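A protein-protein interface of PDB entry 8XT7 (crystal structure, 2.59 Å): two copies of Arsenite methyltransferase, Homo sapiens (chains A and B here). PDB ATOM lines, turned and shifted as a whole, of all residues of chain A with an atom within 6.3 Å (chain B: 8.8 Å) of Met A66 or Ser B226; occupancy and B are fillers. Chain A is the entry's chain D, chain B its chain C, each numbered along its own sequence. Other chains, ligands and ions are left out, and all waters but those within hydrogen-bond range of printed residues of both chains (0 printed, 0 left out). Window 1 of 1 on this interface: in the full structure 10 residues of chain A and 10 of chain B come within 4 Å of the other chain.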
ATOM      1  N   GLY A  41     -21.059  -6.653 -18.359  1.00  0.00           N
ATOM      2  CA  GLY A  41     -21.189  -5.240 -18.640  1.00  0.00           C
ATOM      3  C   GLY A  41     -21.114  -4.903 -20.121  1.00  0.00           C
ATOM      4  O   GLY A  41     -20.304  -4.075 -20.542  1.00  0.00           O
ATOM      5  N   ILE A  64     -24.085  -9.135 -20.994  1.00  0.00           N
ATOM      6  CA  ILE A  64     -25.016  -8.961 -19.900  1.00  0.00           C
ATOM      7  C   ILE A  64     -24.813  -7.556 -19.385  1.00  0.00           C
ATOM      8  O   ILE A  64     -23.670  -7.138 -19.153  1.00  0.00           O
ATOM      9  CB  ILE A  64     -24.804  -9.995 -18.782  1.00  0.00           C
ATOM     10  CG1 ILE A  64     -25.692  -9.637 -17.606  1.00  0.00           C
ATOM     11  CG2 ILE A  64     -23.345 -10.069 -18.335  1.00  0.00           C
ATOM     12  CD1 ILE A  64     -26.541 -10.770 -17.205  1.00  0.00           C
ATOM     13  N   ASP A  65     -25.912  -6.814 -19.274  1.00  0.00           N
ATOM     14  CA  ASP A  65     -25.846  -5.440 -18.803  1.00  0.00           C
ATOM     15  C   ASP A  65     -26.976  -5.208 -17.825  1.00  0.00           C
ATOM     16  O   ASP A  65     -28.063  -5.784 -17.959  1.00  0.00           O
ATOM     17  CB  ASP A  65     -25.918  -4.426 -19.956  1.00  0.00           C
ATOM     18  CG  ASP A  65     -25.470  -3.038 -19.525  1.00  0.00           C
ATOM     19  OD1 ASP A  65     -24.253  -2.860 -19.301  1.00  0.00           O
ATOM     20  OD2 ASP A  65     -26.330  -2.136 -19.386  1.00  0.00           O
ATOM     21  N   MET A  66     -26.711  -4.371 -16.823  1.00  0.00           N
ATOM     22  CA  MET A  66     -27.766  -4.156 -15.844  1.00  0.00           C
ATOM     23  C   MET A  66     -28.800  -3.148 -16.304  1.00  0.00           C
ATOM     24  O   MET A  66     -29.805  -2.988 -15.623  1.00  0.00           O
ATOM     25  CB  MET A  66     -27.206  -3.697 -14.505  1.00  0.00           C
ATOM     26  CG  MET A  66     -26.661  -2.317 -14.508  1.00  0.00           C
ATOM     27  SD  MET A  66     -25.979  -1.960 -12.886  1.00  0.00           S
ATOM     28  CE  MET A  66     -25.175  -0.372 -13.210  1.00  0.00           C
ATOM     29  N   THR A  67     -28.605  -2.504 -17.445  1.00  0.00           N
ATOM     30  CA  THR A  67     -29.467  -1.420 -17.897  1.00  0.00           C
ATOM     31  C   THR A  67     -30.251  -1.862 -19.121  1.00  0.00           C
ATOM     32  O   THR A  67     -29.686  -1.958 -20.220  1.00  0.00           O
ATOM     33  CB  THR A  67     -28.633  -0.189 -18.213  1.00  0.00           C
ATOM     34  OG1 THR A  67     -28.129   0.356 -16.990  1.00  0.00           O
ATOM     35  CG2 THR A  67     -29.482   0.809 -18.911  1.00  0.00           C
ATOM     36  N   LYS A  68     -31.568  -2.068 -18.939  1.00  0.00           N
ATOM     37  CA  LYS A  68     -32.418  -2.607 -20.003  1.00  0.00           C
ATOM     38  C   LYS A  68     -32.313  -1.781 -21.285  1.00  0.00           C
ATOM     39  O   LYS A  68     -32.350  -2.323 -22.393  1.00  0.00           O
ATOM     40  CB  LYS A  68     -33.872  -2.678 -19.512  1.00  0.00           C
ATOM     41  CG  LYS A  68     -34.819  -3.523 -20.372  1.00  0.00           C
ATOM     42  CD  LYS A  68     -36.196  -3.671 -19.702  1.00  0.00           C
ATOM     43  CE  LYS A  68     -36.133  -4.373 -18.310  1.00  0.00           C
ATOM     44  NZ  LYS A  68     -37.384  -4.293 -17.423  1.00  0.00           N
ATOM     45  N   VAL A  71     -29.396  -2.785 -23.312  1.00  0.00           N
ATOM     46  CA  VAL A  71     -29.614  -4.065 -23.971  1.00  0.00           C
ATOM     47  C   VAL A  71     -30.484  -3.865 -25.202  1.00  0.00           C
ATOM     48  O   VAL A  71     -30.234  -4.448 -26.269  1.00  0.00           O
ATOM     49  CB  VAL A  71     -30.221  -5.082 -22.983  1.00  0.00           C
ATOM     50  CG1 VAL A  71     -30.682  -6.307 -23.723  1.00  0.00           C
ATOM     51  CG2 VAL A  71     -29.212  -5.460 -21.848  1.00  0.00           C
ATOM     52  N   ILE A  95     -28.319 -10.008 -22.715  1.00  0.00           N
ATOM     53  CA  ILE A  95     -29.144 -10.297 -21.566  1.00  0.00           C
ATOM     54  C   ILE A  95     -29.202  -9.057 -20.685  1.00  0.00           C
ATOM     55  O   ILE A  95     -28.186  -8.379 -20.476  1.00  0.00           O
ATOM     56  CB  ILE A  95     -28.562 -11.491 -20.800  1.00  0.00           C
ATOM     57  CG1 ILE A  95     -28.604 -12.738 -21.683  1.00  0.00           C
ATOM     58  CG2 ILE A  95     -29.307 -11.694 -19.531  1.00  0.00           C
ATOM     59  CD1 ILE A  95     -27.846 -13.888 -21.070  1.00  0.00           C
ATOM     60  N   HIS A  96     -30.394  -8.739 -20.198  1.00  0.00           N
ATOM     61  CA  HIS A  96     -30.522  -7.755 -19.138  1.00  0.00           C
ATOM     62  C   HIS A  96     -30.477  -8.507 -17.809  1.00  0.00           C
ATOM     63  O   HIS A  96     -31.339  -9.352 -17.537  1.00  0.00           O
ATOM     64  CB  HIS A  96     -31.802  -6.923 -19.275  1.00  0.00           C
ATOM     65  CG  HIS A  96     -31.963  -5.922 -18.174  1.00  0.00           C
ATOM     66  ND1 HIS A  96     -33.187  -5.477 -17.724  1.00  0.00           N
ATOM     67  CD2 HIS A  96     -31.035  -5.330 -17.388  1.00  0.00           C
ATOM     68  CE1 HIS A  96     -33.002  -4.631 -16.726  1.00  0.00           C
ATOM     69  NE2 HIS A  96     -31.705  -4.529 -16.501  1.00  0.00           N
ATOM     70  N   GLY A  97     -29.449  -8.230 -17.012  1.00  0.00           N
ATOM     71  CA  GLY A  97     -29.224  -8.956 -15.774  1.00  0.00           C
ATOM     72  C   GLY A  97     -28.130  -8.284 -14.977  1.00  0.00           C
ATOM     73  O   GLY A  97     -27.385  -7.445 -15.495  1.00  0.00           O
ATOM     74  N   TYR A  98     -28.051  -8.665 -13.712  1.00  0.00           N
ATOM     75  CA  TYR A  98     -27.059  -8.133 -12.783  1.00  0.00           C
ATOM     76  C   TYR A  98     -25.893  -9.112 -12.721  1.00  0.00           C
ATOM     77  O   TYR A  98     -26.091 -10.338 -12.667  1.00  0.00           O
ATOM     78  CB  TYR A  98     -27.623  -7.932 -11.367  1.00  0.00           C
ATOM     79  CG  TYR A  98     -28.894  -7.119 -11.197  1.00  0.00           C
ATOM     80  CD1 TYR A  98     -29.427  -6.373 -12.248  1.00  0.00           C
ATOM     81  CD2 TYR A  98     -29.547  -7.082  -9.954  1.00  0.00           C
ATOM     82  CE1 TYR A  98     -30.583  -5.629 -12.080  1.00  0.00           C
ATOM     83  CE2 TYR A  98     -30.702  -6.336  -9.775  1.00  0.00           C
ATOM     84  CZ  TYR A  98     -31.215  -5.612 -10.847  1.00  0.00           C
ATOM     85  OH  TYR A  98     -32.363  -4.865 -10.698  1.00  0.00           O
ATOM     86  N   ILE A  99     -24.665  -8.578 -12.723  1.00  0.00           N
ATOM     87  CA  ILE A  99     -23.554  -9.492 -12.956  1.00  0.00           C
ATOM     88  C   ILE A  99     -23.313 -10.360 -11.729  1.00  0.00           C
ATOM     89  O   ILE A  99     -22.889 -11.515 -11.861  1.00  0.00           O
ATOM     90  CB  ILE A  99     -22.274  -8.757 -13.395  1.00  0.00           C
ATOM     91  CG1 ILE A  99     -21.684  -7.945 -12.248  1.00  0.00           C
ATOM     92  CG2 ILE A  99     -22.511  -7.912 -14.667  1.00  0.00           C
ATOM     93  CD1 ILE A  99     -20.194  -7.938 -12.275  1.00  0.00           C
ATOM     94  N   ASN B 109     -38.730  -7.417 -11.045  1.00  0.00           N
ATOM     95  CA  ASN B 109     -37.618  -6.433 -11.005  1.00  0.00           C
ATOM     96  C   ASN B 109     -37.921  -5.315 -12.003  1.00  0.00           C
ATOM     97  O   ASN B 109     -38.514  -5.623 -13.055  1.00  0.00           O
ATOM     98  CB  ASN B 109     -36.276  -7.057 -11.400  1.00  0.00           C
ATOM     99  CG  ASN B 109     -36.114  -8.508 -10.997  1.00  0.00           C
ATOM    100  OD1 ASN B 109     -35.516  -8.806  -9.967  1.00  0.00           O
ATOM    101  ND2 ASN B 109     -36.609  -9.418 -11.819  1.00  0.00           N
ATOM    102  N   GLU B 110     -37.539  -4.075 -11.686  1.00  0.00           N
ATOM    103  CA  GLU B 110     -37.705  -2.949 -12.647  1.00  0.00           C
ATOM    104  C   GLU B 110     -39.155  -2.888 -13.142  1.00  0.00           C
ATOM    105  O   GLU B 110     -39.354  -2.795 -14.367  1.00  0.00           O
ATOM    106  CB  GLU B 110     -36.671  -3.033 -13.770  1.00  0.00           C
ATOM    107  CG  GLU B 110     -35.242  -3.009 -13.262  1.00  0.00           C
ATOM    108  CD  GLU B 110     -34.208  -2.567 -14.281  1.00  0.00           C
ATOM    109  OE1 GLU B 110     -34.609  -2.148 -15.383  1.00  0.00           O
ATOM    110  OE2 GLU B 110     -33.004  -2.643 -13.968  1.00  0.00           O
ATOM    111  N   TYR B 135     -34.789  -1.222  -4.216  1.00  0.00           N
ATOM    112  CA  TYR B 135     -33.861  -1.035  -5.359  1.00  0.00           C
ATOM    113  C   TYR B 135     -34.237  -2.004  -6.482  1.00  0.00           C
ATOM    114  O   TYR B 135     -34.369  -1.557  -7.625  1.00  0.00           O
ATOM    115  CB  TYR B 135     -32.419  -1.277  -4.912  1.00  0.00           C
ATOM    116  CG  TYR B 135     -31.393  -1.186  -6.012  1.00  0.00           C
ATOM    117  CD1 TYR B 135     -30.893  -2.327  -6.618  1.00  0.00           C
ATOM    118  CD2 TYR B 135     -30.922   0.039  -6.448  1.00  0.00           C
ATOM    119  CE1 TYR B 135     -29.953  -2.251  -7.633  1.00  0.00           C
ATOM    120  CE2 TYR B 135     -29.982   0.131  -7.459  1.00  0.00           C
ATOM    121  CZ  TYR B 135     -29.495  -1.017  -8.054  1.00  0.00           C
ATOM    122  OH  TYR B 135     -28.568  -0.932  -9.052  1.00  0.00           O
ATOM    123  N   LEU B 138     -37.534  -1.240  -8.394  1.00  0.00           N
ATOM    124  CA  LEU B 138     -37.526   0.073  -9.027  1.00  0.00           C
ATOM    125  C   LEU B 138     -36.954   0.022 -10.457  1.00  0.00           C
ATOM    126  O   LEU B 138     -35.905  -0.586 -10.701  1.00  0.00           O
ATOM    127  CB  LEU B 138     -36.699   1.004  -8.159  1.00  0.00           C
ATOM    128  CG  LEU B 138     -37.365   1.732  -7.009  1.00  0.00           C
ATOM    129  CD1 LEU B 138     -36.349   2.675  -6.435  1.00  0.00           C
ATOM    130  CD2 LEU B 138     -38.605   2.478  -7.430  1.00  0.00           C
ATOM    131  N   LYS B 139     -37.663   0.630 -11.409  1.00  0.00           N
ATOM    132  CA  LYS B 139     -37.125   0.851 -12.754  1.00  0.00           C
ATOM    133  C   LYS B 139     -35.899   1.779 -12.722  1.00  0.00           C
ATOM    134  O   LYS B 139     -35.630   2.471 -11.740  1.00  0.00           O
ATOM    135  CB  LYS B 139     -38.197   1.465 -13.671  1.00  0.00           C
ATOM    136  CG  LYS B 139     -39.343   0.515 -14.029  1.00  0.00           C
ATOM    137  CD  LYS B 139     -40.649   1.232 -14.396  1.00  0.00           C
ATOM    138  CE  LYS B 139     -40.814   1.580 -15.866  1.00  0.00           C
ATOM    139  NZ  LYS B 139     -42.268   1.772 -16.233  1.00  0.00           N
ATOM    140  N   HIS B 140     -35.139   1.768 -13.811  1.00  0.00           N
ATOM    141  CA  HIS B 140     -34.074   2.752 -14.003  1.00  0.00           C
ATOM    142  C   HIS B 140     -34.652   4.154 -13.954  1.00  0.00           C
ATOM    143  O   HIS B 140     -35.651   4.440 -14.619  1.00  0.00           O
ATOM    144  CB  HIS B 140     -33.378   2.538 -15.357  1.00  0.00           C
ATOM    145  CG  HIS B 140     -32.164   3.389 -15.562  1.00  0.00           C
ATOM    146  ND1 HIS B 140     -32.136   4.445 -16.449  1.00  0.00           N
ATOM    147  CD2 HIS B 140     -30.933   3.339 -15.001  1.00  0.00           C
ATOM    148  CE1 HIS B 140     -30.943   5.011 -16.421  1.00  0.00           C
ATOM    149  NE2 HIS B 140     -30.193   4.361 -15.549  1.00  0.00           N
ATOM    150  N   GLY B 141     -34.008   5.033 -13.189  1.00  0.00           N
ATOM    151  CA  GLY B 141     -34.485   6.393 -12.999  1.00  0.00           C
ATOM    152  C   GLY B 141     -35.613   6.559 -12.001  1.00  0.00           C
ATOM    153  O   GLY B 141     -36.098   7.685 -11.825  1.00  0.00           O
ATOM    154  N   GLY B 142     -36.051   5.469 -11.341  1.00  0.00           N
ATOM    155  CA  GLY B 142     -37.121   5.544 -10.369  1.00  0.00           C
ATOM    156  C   GLY B 142     -36.628   5.967  -9.016  1.00  0.00           C
ATOM    157  O   GLY B 142     -35.422   6.085  -8.776  1.00  0.00           O
ATOM    158  N   ILE B 186     -25.916  -0.461  -1.898  1.00  0.00           N
ATOM    159  CA  ILE B 186     -27.027  -1.138  -2.556  1.00  0.00           C
ATOM    160  C   ILE B 186     -27.108  -0.765  -4.037  1.00  0.00           C
ATOM    161  O   ILE B 186     -27.524  -1.588  -4.863  1.00  0.00           O
ATOM    162  CB  ILE B 186     -28.348  -0.831  -1.817  1.00  0.00           C
ATOM    163  CG1 ILE B 186     -28.337  -1.453  -0.425  1.00  0.00           C
ATOM    164  CG2 ILE B 186     -29.602  -1.287  -2.637  1.00  0.00           C
ATOM    165  CD1 ILE B 186     -29.704  -1.512   0.275  1.00  0.00           C
ATOM    166  N   GLY B 187     -26.727   0.463  -4.390  1.00  0.00           N
ATOM    167  CA  GLY B 187     -26.833   0.926  -5.758  1.00  0.00           C
ATOM    168  C   GLY B 187     -27.625   2.210  -5.921  1.00  0.00           C
ATOM    169  O   GLY B 187     -27.854   2.652  -7.041  1.00  0.00           O
ATOM    170  N   PHE B 188     -28.075   2.810  -4.829  1.00  0.00           N
ATOM    171  CA  PHE B 188     -28.750   4.092  -4.923  1.00  0.00           C
ATOM    172  C   PHE B 188     -27.736   5.217  -5.057  1.00  0.00           C
ATOM    173  O   PHE B 188     -26.598   5.123  -4.574  1.00  0.00           O
ATOM    174  CB  PHE B 188     -29.643   4.366  -3.687  1.00  0.00           C
ATOM    175  CG  PHE B 188     -30.941   3.591  -3.670  1.00  0.00           C
ATOM    176  CD1 PHE B 188     -31.897   3.765  -4.680  1.00  0.00           C
ATOM    177  CD2 PHE B 188     -31.204   2.661  -2.667  1.00  0.00           C
ATOM    178  CE1 PHE B 188     -33.102   3.027  -4.685  1.00  0.00           C
ATOM    179  CE2 PHE B 188     -32.410   1.911  -2.659  1.00  0.00           C
ATOM    180  CZ  PHE B 188     -33.358   2.093  -3.663  1.00  0.00           C
ATOM    181  N   CYS B 189     -28.173   6.308  -5.716  1.00  0.00           N
ATOM    182  CA  CYS B 189     -27.478   7.598  -5.677  1.00  0.00           C
ATOM    183  C   CYS B 189     -27.485   8.070  -4.234  1.00  0.00           C
ATOM    184  O   CYS B 189     -28.195   7.498  -3.396  1.00  0.00           O
ATOM    185  CB  CYS B 189     -28.173   8.629  -6.565  1.00  0.00           C
ATOM    186  SG  CYS B 189     -28.263   8.175  -8.310  1.00  0.00           S
ATOM    187  N   PHE B 223     -32.602   7.629  -5.544  1.00  0.00           N
ATOM    188  CA  PHE B 223     -32.780   7.326  -6.958  1.00  0.00           C
ATOM    189  C   PHE B 223     -31.926   6.142  -7.393  1.00  0.00           C
ATOM    190  O   PHE B 223     -30.827   5.886  -6.878  1.00  0.00           O
ATOM    191  CB  PHE B 223     -32.467   8.549  -7.825  1.00  0.00           C
ATOM    192  CG  PHE B 223     -33.552   9.592  -7.809  1.00  0.00           C
ATOM    193  CD1 PHE B 223     -34.646   9.495  -8.676  1.00  0.00           C
ATOM    194  CD2 PHE B 223     -33.486  10.669  -6.923  1.00  0.00           C
ATOM    195  CE1 PHE B 223     -35.656  10.465  -8.662  1.00  0.00           C
ATOM    196  CE2 PHE B 223     -34.480  11.648  -6.895  1.00  0.00           C
ATOM    197  CZ  PHE B 223     -35.571  11.547  -7.768  1.00  0.00           C
ATOM    198  N   LYS B 224     -32.460   5.413  -8.346  1.00  0.00           N
ATOM    199  CA  LYS B 224     -31.786   4.269  -8.937  1.00  0.00           C
ATOM    200  C   LYS B 224     -31.477   4.623 -10.385  1.00  0.00           C
ATOM    201  O   LYS B 224     -32.398   4.792 -11.191  1.00  0.00           O
ATOM    202  CB  LYS B 224     -32.675   3.033  -8.843  1.00  0.00           C
ATOM    203  CG  LYS B 224     -32.151   1.875  -9.649  1.00  0.00           C
ATOM    204  CD  LYS B 224     -33.171   0.778  -9.718  1.00  0.00           C
ATOM    205  CE  LYS B 224     -32.528  -0.490 -10.221  1.00  0.00           C
ATOM    206  NZ  LYS B 224     -33.454  -1.644 -10.093  1.00  0.00           N
ATOM    207  N   HIS B 225     -30.195   4.769 -10.720  1.00  0.00           N
ATOM    208  CA  HIS B 225     -29.849   4.838 -12.139  1.00  0.00           C
ATOM    209  C   HIS B 225     -28.390   4.444 -12.343  1.00  0.00           C
ATOM    210  O   HIS B 225     -27.625   4.285 -11.385  1.00  0.00           O
ATOM    211  CB  HIS B 225     -30.158   6.217 -12.744  1.00  0.00           C
ATOM    212  CG  HIS B 225     -29.310   7.334 -12.220  1.00  0.00           C
ATOM    213  ND1 HIS B 225     -27.933   7.304 -12.239  1.00  0.00           N
ATOM    214  CD2 HIS B 225     -29.649   8.537 -11.705  1.00  0.00           C
ATOM    215  CE1 HIS B 225     -27.459   8.428 -11.733  1.00  0.00           C
ATOM    216  NE2 HIS B 225     -28.482   9.195 -11.402  1.00  0.00           N
ATOM    217  N   SER B 226     -28.030   4.282 -13.621  1.00  0.00           N
ATOM    218  CA  SER B 226     -26.773   3.685 -14.058  1.00  0.00           C
ATOM    219  C   SER B 226     -25.991   4.691 -14.890  1.00  0.00           C
ATOM    220  O   SER B 226     -26.576   5.564 -15.537  1.00  0.00           O
ATOM    221  CB  SER B 226     -27.015   2.408 -14.892  1.00  0.00           C
ATOM    222  OG  SER B 226     -27.962   1.555 -14.266  1.00  0.00           O
ATOM    223  N   LYS B 227     -24.658   4.538 -14.892  1.00  0.00           N
ATOM    224  CA  LYS B 227     -23.745   5.508 -15.514  1.00  0.00           C
ATOM    225  C   LYS B 227     -23.341   5.025 -16.907  1.00  0.00           C
ATOM    226  O   LYS B 227     -22.285   4.424 -17.121  1.00  0.00           O
ATOM    227  CB  LYS B 227     -22.528   5.742 -14.626  1.00  0.00           C
ATOM    228  CG  LYS B 227     -21.737   6.983 -14.977  1.00  0.00           C
ATOM    229  CD  LYS B 227     -20.509   7.113 -14.095  1.00  0.00           C
ATOM    230  CE  LYS B 227     -20.215   8.576 -13.794  1.00  0.00           C
ATOM    231  NZ  LYS B 227     -19.961   9.357 -15.034  1.00  0.00           N
ATOM    232  N   THR B 228     -24.201   5.335 -17.878  1.00  0.00           N
ATOM    233  CA  THR B 228     -24.042   4.936 -19.273  1.00  0.00           C
ATOM    234  C   THR B 228     -22.970   5.738 -20.017  1.00  0.00           C
ATOM    235  O   THR B 228     -22.656   5.417 -21.176  1.00  0.00           O
ATOM    236  CB  THR B 228     -25.403   5.068 -19.971  1.00  0.00           C
ATOM    237  OG1 THR B 228     -25.212   5.421 -21.345  1.00  0.00           O
ATOM    238  CG2 THR B 228     -26.263   6.139 -19.282  1.00  0.00           C
ATOM    239  N   GLY B 229     -22.381   6.745 -19.383  1.00  0.00           N
ATOM    240  CA  GLY B 229     -21.497   7.650 -20.069  1.00  0.00           C
ATOM    241  C   GLY B 229     -21.065   8.758 -19.143  1.00  0.00           C
ATOM    242  O   GLY B 229     -21.562   8.891 -18.022  1.00  0.00           O
ATOM    243  N   PRO B 230     -20.120   9.573 -19.589  1.00  0.00           N
ATOM    244  CA  PRO B 230     -19.684  10.691 -18.754  1.00  0.00           C
ATOM    245  C   PRO B 230     -20.809  11.699 -18.604  1.00  0.00           C
ATOM    246  O   PRO B 230     -21.666  11.850 -19.477  1.00  0.00           O
ATOM    247  CB  PRO B 230     -18.494  11.272 -19.526  1.00  0.00           C
ATOM    248  CG  PRO B 230     -18.763  10.905 -20.955  1.00  0.00           C
ATOM    249  CD  PRO B 230     -19.528   9.607 -20.938  1.00  0.00           C
ATOM    250  N   THR B 231     -20.822  12.360 -17.457  1.00  0.00           N
ATOM    251  CA  THR B 231     -21.794  13.400 -17.161  1.00  0.00           C
ATOM    252  C   THR B 231     -21.015  14.675 -16.893  1.00  0.00           C
ATOM    253  O   THR B 231     -20.003  14.645 -16.182  1.00  0.00           O
ATOM    254  CB  THR B 231     -22.669  13.003 -15.959  1.00  0.00           C
ATOM    255  OG1 THR B 231     -22.177  13.607 -14.760  1.00  0.00           O
ATOM    256  CG2 THR B 231     -22.635  11.495 -15.769  1.00  0.00           C
ATOM    257  N   ALA B 271     -27.661  13.977 -13.552  1.00  0.00           N
ATOM    258  CA  ALA B 271     -27.949  12.597 -13.930  1.00  0.00           C
ATOM    259  C   ALA B 271     -29.329  12.190 -13.459  1.00  0.00           C
ATOM    260  O   ALA B 271     -30.088  11.552 -14.204  1.00  0.00           O
ATOM    261  CB  ALA B 271     -26.884  11.668 -13.345  1.00  0.00           C
ATOM    262  N   ILE B 272     -29.675  12.578 -12.231  1.00  0.00           N
ATOM    263  CA  ILE B 272     -30.987  12.218 -11.694  1.00  0.00           C
ATOM    264  C   ILE B 272     -32.087  12.864 -12.520  1.00  0.00           C
ATOM    265  O   ILE B 272     -33.047  12.199 -12.927  1.00  0.00           O
ATOM    266  CB  ILE B 272     -31.121  12.606 -10.218  1.00  0.00           C
ATOM    267  CG1 ILE B 272     -30.187  11.767  -9.344  1.00  0.00           C
ATOM    268  CG2 ILE B 272     -32.558  12.390  -9.804  1.00  0.00           C
ATOM    269  CD1 ILE B 272     -29.946  12.387  -7.959  1.00  0.00           C
ATOM    270  N   ASN B 275     -32.228  11.163 -16.033  1.00  0.00           N
ATOM    271  CA  ASN B 275     -32.613   9.765 -16.120  1.00  0.00           C
ATOM    272  C   ASN B 275     -33.970   9.449 -15.521  1.00  0.00           C
ATOM    273  O   ASN B 275     -34.531   8.391 -15.824  1.00  0.00           O
ATOM    274  CB  ASN B 275     -31.540   8.918 -15.454  1.00  0.00           C
ATOM    275  CG  ASN B 275     -30.311   8.847 -16.297  1.00  0.00           C
ATOM    276  OD1 ASN B 275     -30.287   8.122 -17.303  1.00  0.00           O
ATOM    277  ND2 ASN B 275     -29.297   9.632 -15.940  1.00  0.00           N
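No position is printed for both chains.
A ring nitrogen (NE2) of His A96 sits close to the side-chain carboxylate (OE2) of Glu B110 (3.4 Å). The side-chain amino group (NZ) of Lys B224 sits at hydrogen-bond distance from the side-chain hydroxyl (OH) of Tyr A98 (3.5 Å). OG of Ser B226 is in hydrogen-bond range of OG1 of Thr A67, 3.0 Å away.
The backbone carbonyl oxygen (O) of Tyr B135 sits at hydrogen-bond distance from the side-chain amino group (NZ) of Lys B224 (2.6 Å). NZ of Lys B224 is in hydrogen-bond range of O of Leu B138 (2.7 Å). A ring nitrogen (NE2) of His B140 lies within hydrogen-bond range of the backbone NH (N) of Ser B226 (2.9 Å). The backbone NH (N) of Lys B224 is in hydrogen-bond range of the backbone carbonyl oxygen (O) of Gly B142. The backbone NH of Met A66 sits close to the backbone carbonyl oxygen of Gly A97 (3.4 Å). NE2 of His A96 is in hydrogen-bond range of N of Lys A68.
Among the printed residues, pairs that only touch across the chains: Met A66 with Ser B226 (3.5 Å), Met A66 with Glu B110 (3.6 Å) and Lys A68 with Glu B110 (3.9 Å).
Of chain B, only Glu B110 (3.6 Å) and Ser B226 (3.5 Å) come within 4 Å of Met A66. Of chain A, only Met A66 and Thr A67 come within 4 Å of Ser B226. No residue of chain B comes within 4 Å of Asp A65. Printed residues of chain B within 4 Å of Lys A68: Glu B110 (3.9 Å). Printed residues of chain B within 4 Å of Thr A67: Ser B226 (3.0 Å). Of the printed residues of chain A, Glu B110 touches Met A66 (3.6 Å), Lys A68 (3.9 Å) and His A96 (3.2 Å). Ile A64 touches none of the printed residues of chain B.
Printed residues of chain B that touch a printed residue of chain A: Glu B110, Lys B224 and Ser B226. Among the printed residues, 6 pairs touch across the chains. Among the printed residues, no Asp or Glu carboxylate lies within 4 Å of a Lys or Arg side-chain nitrogen of the other chain.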
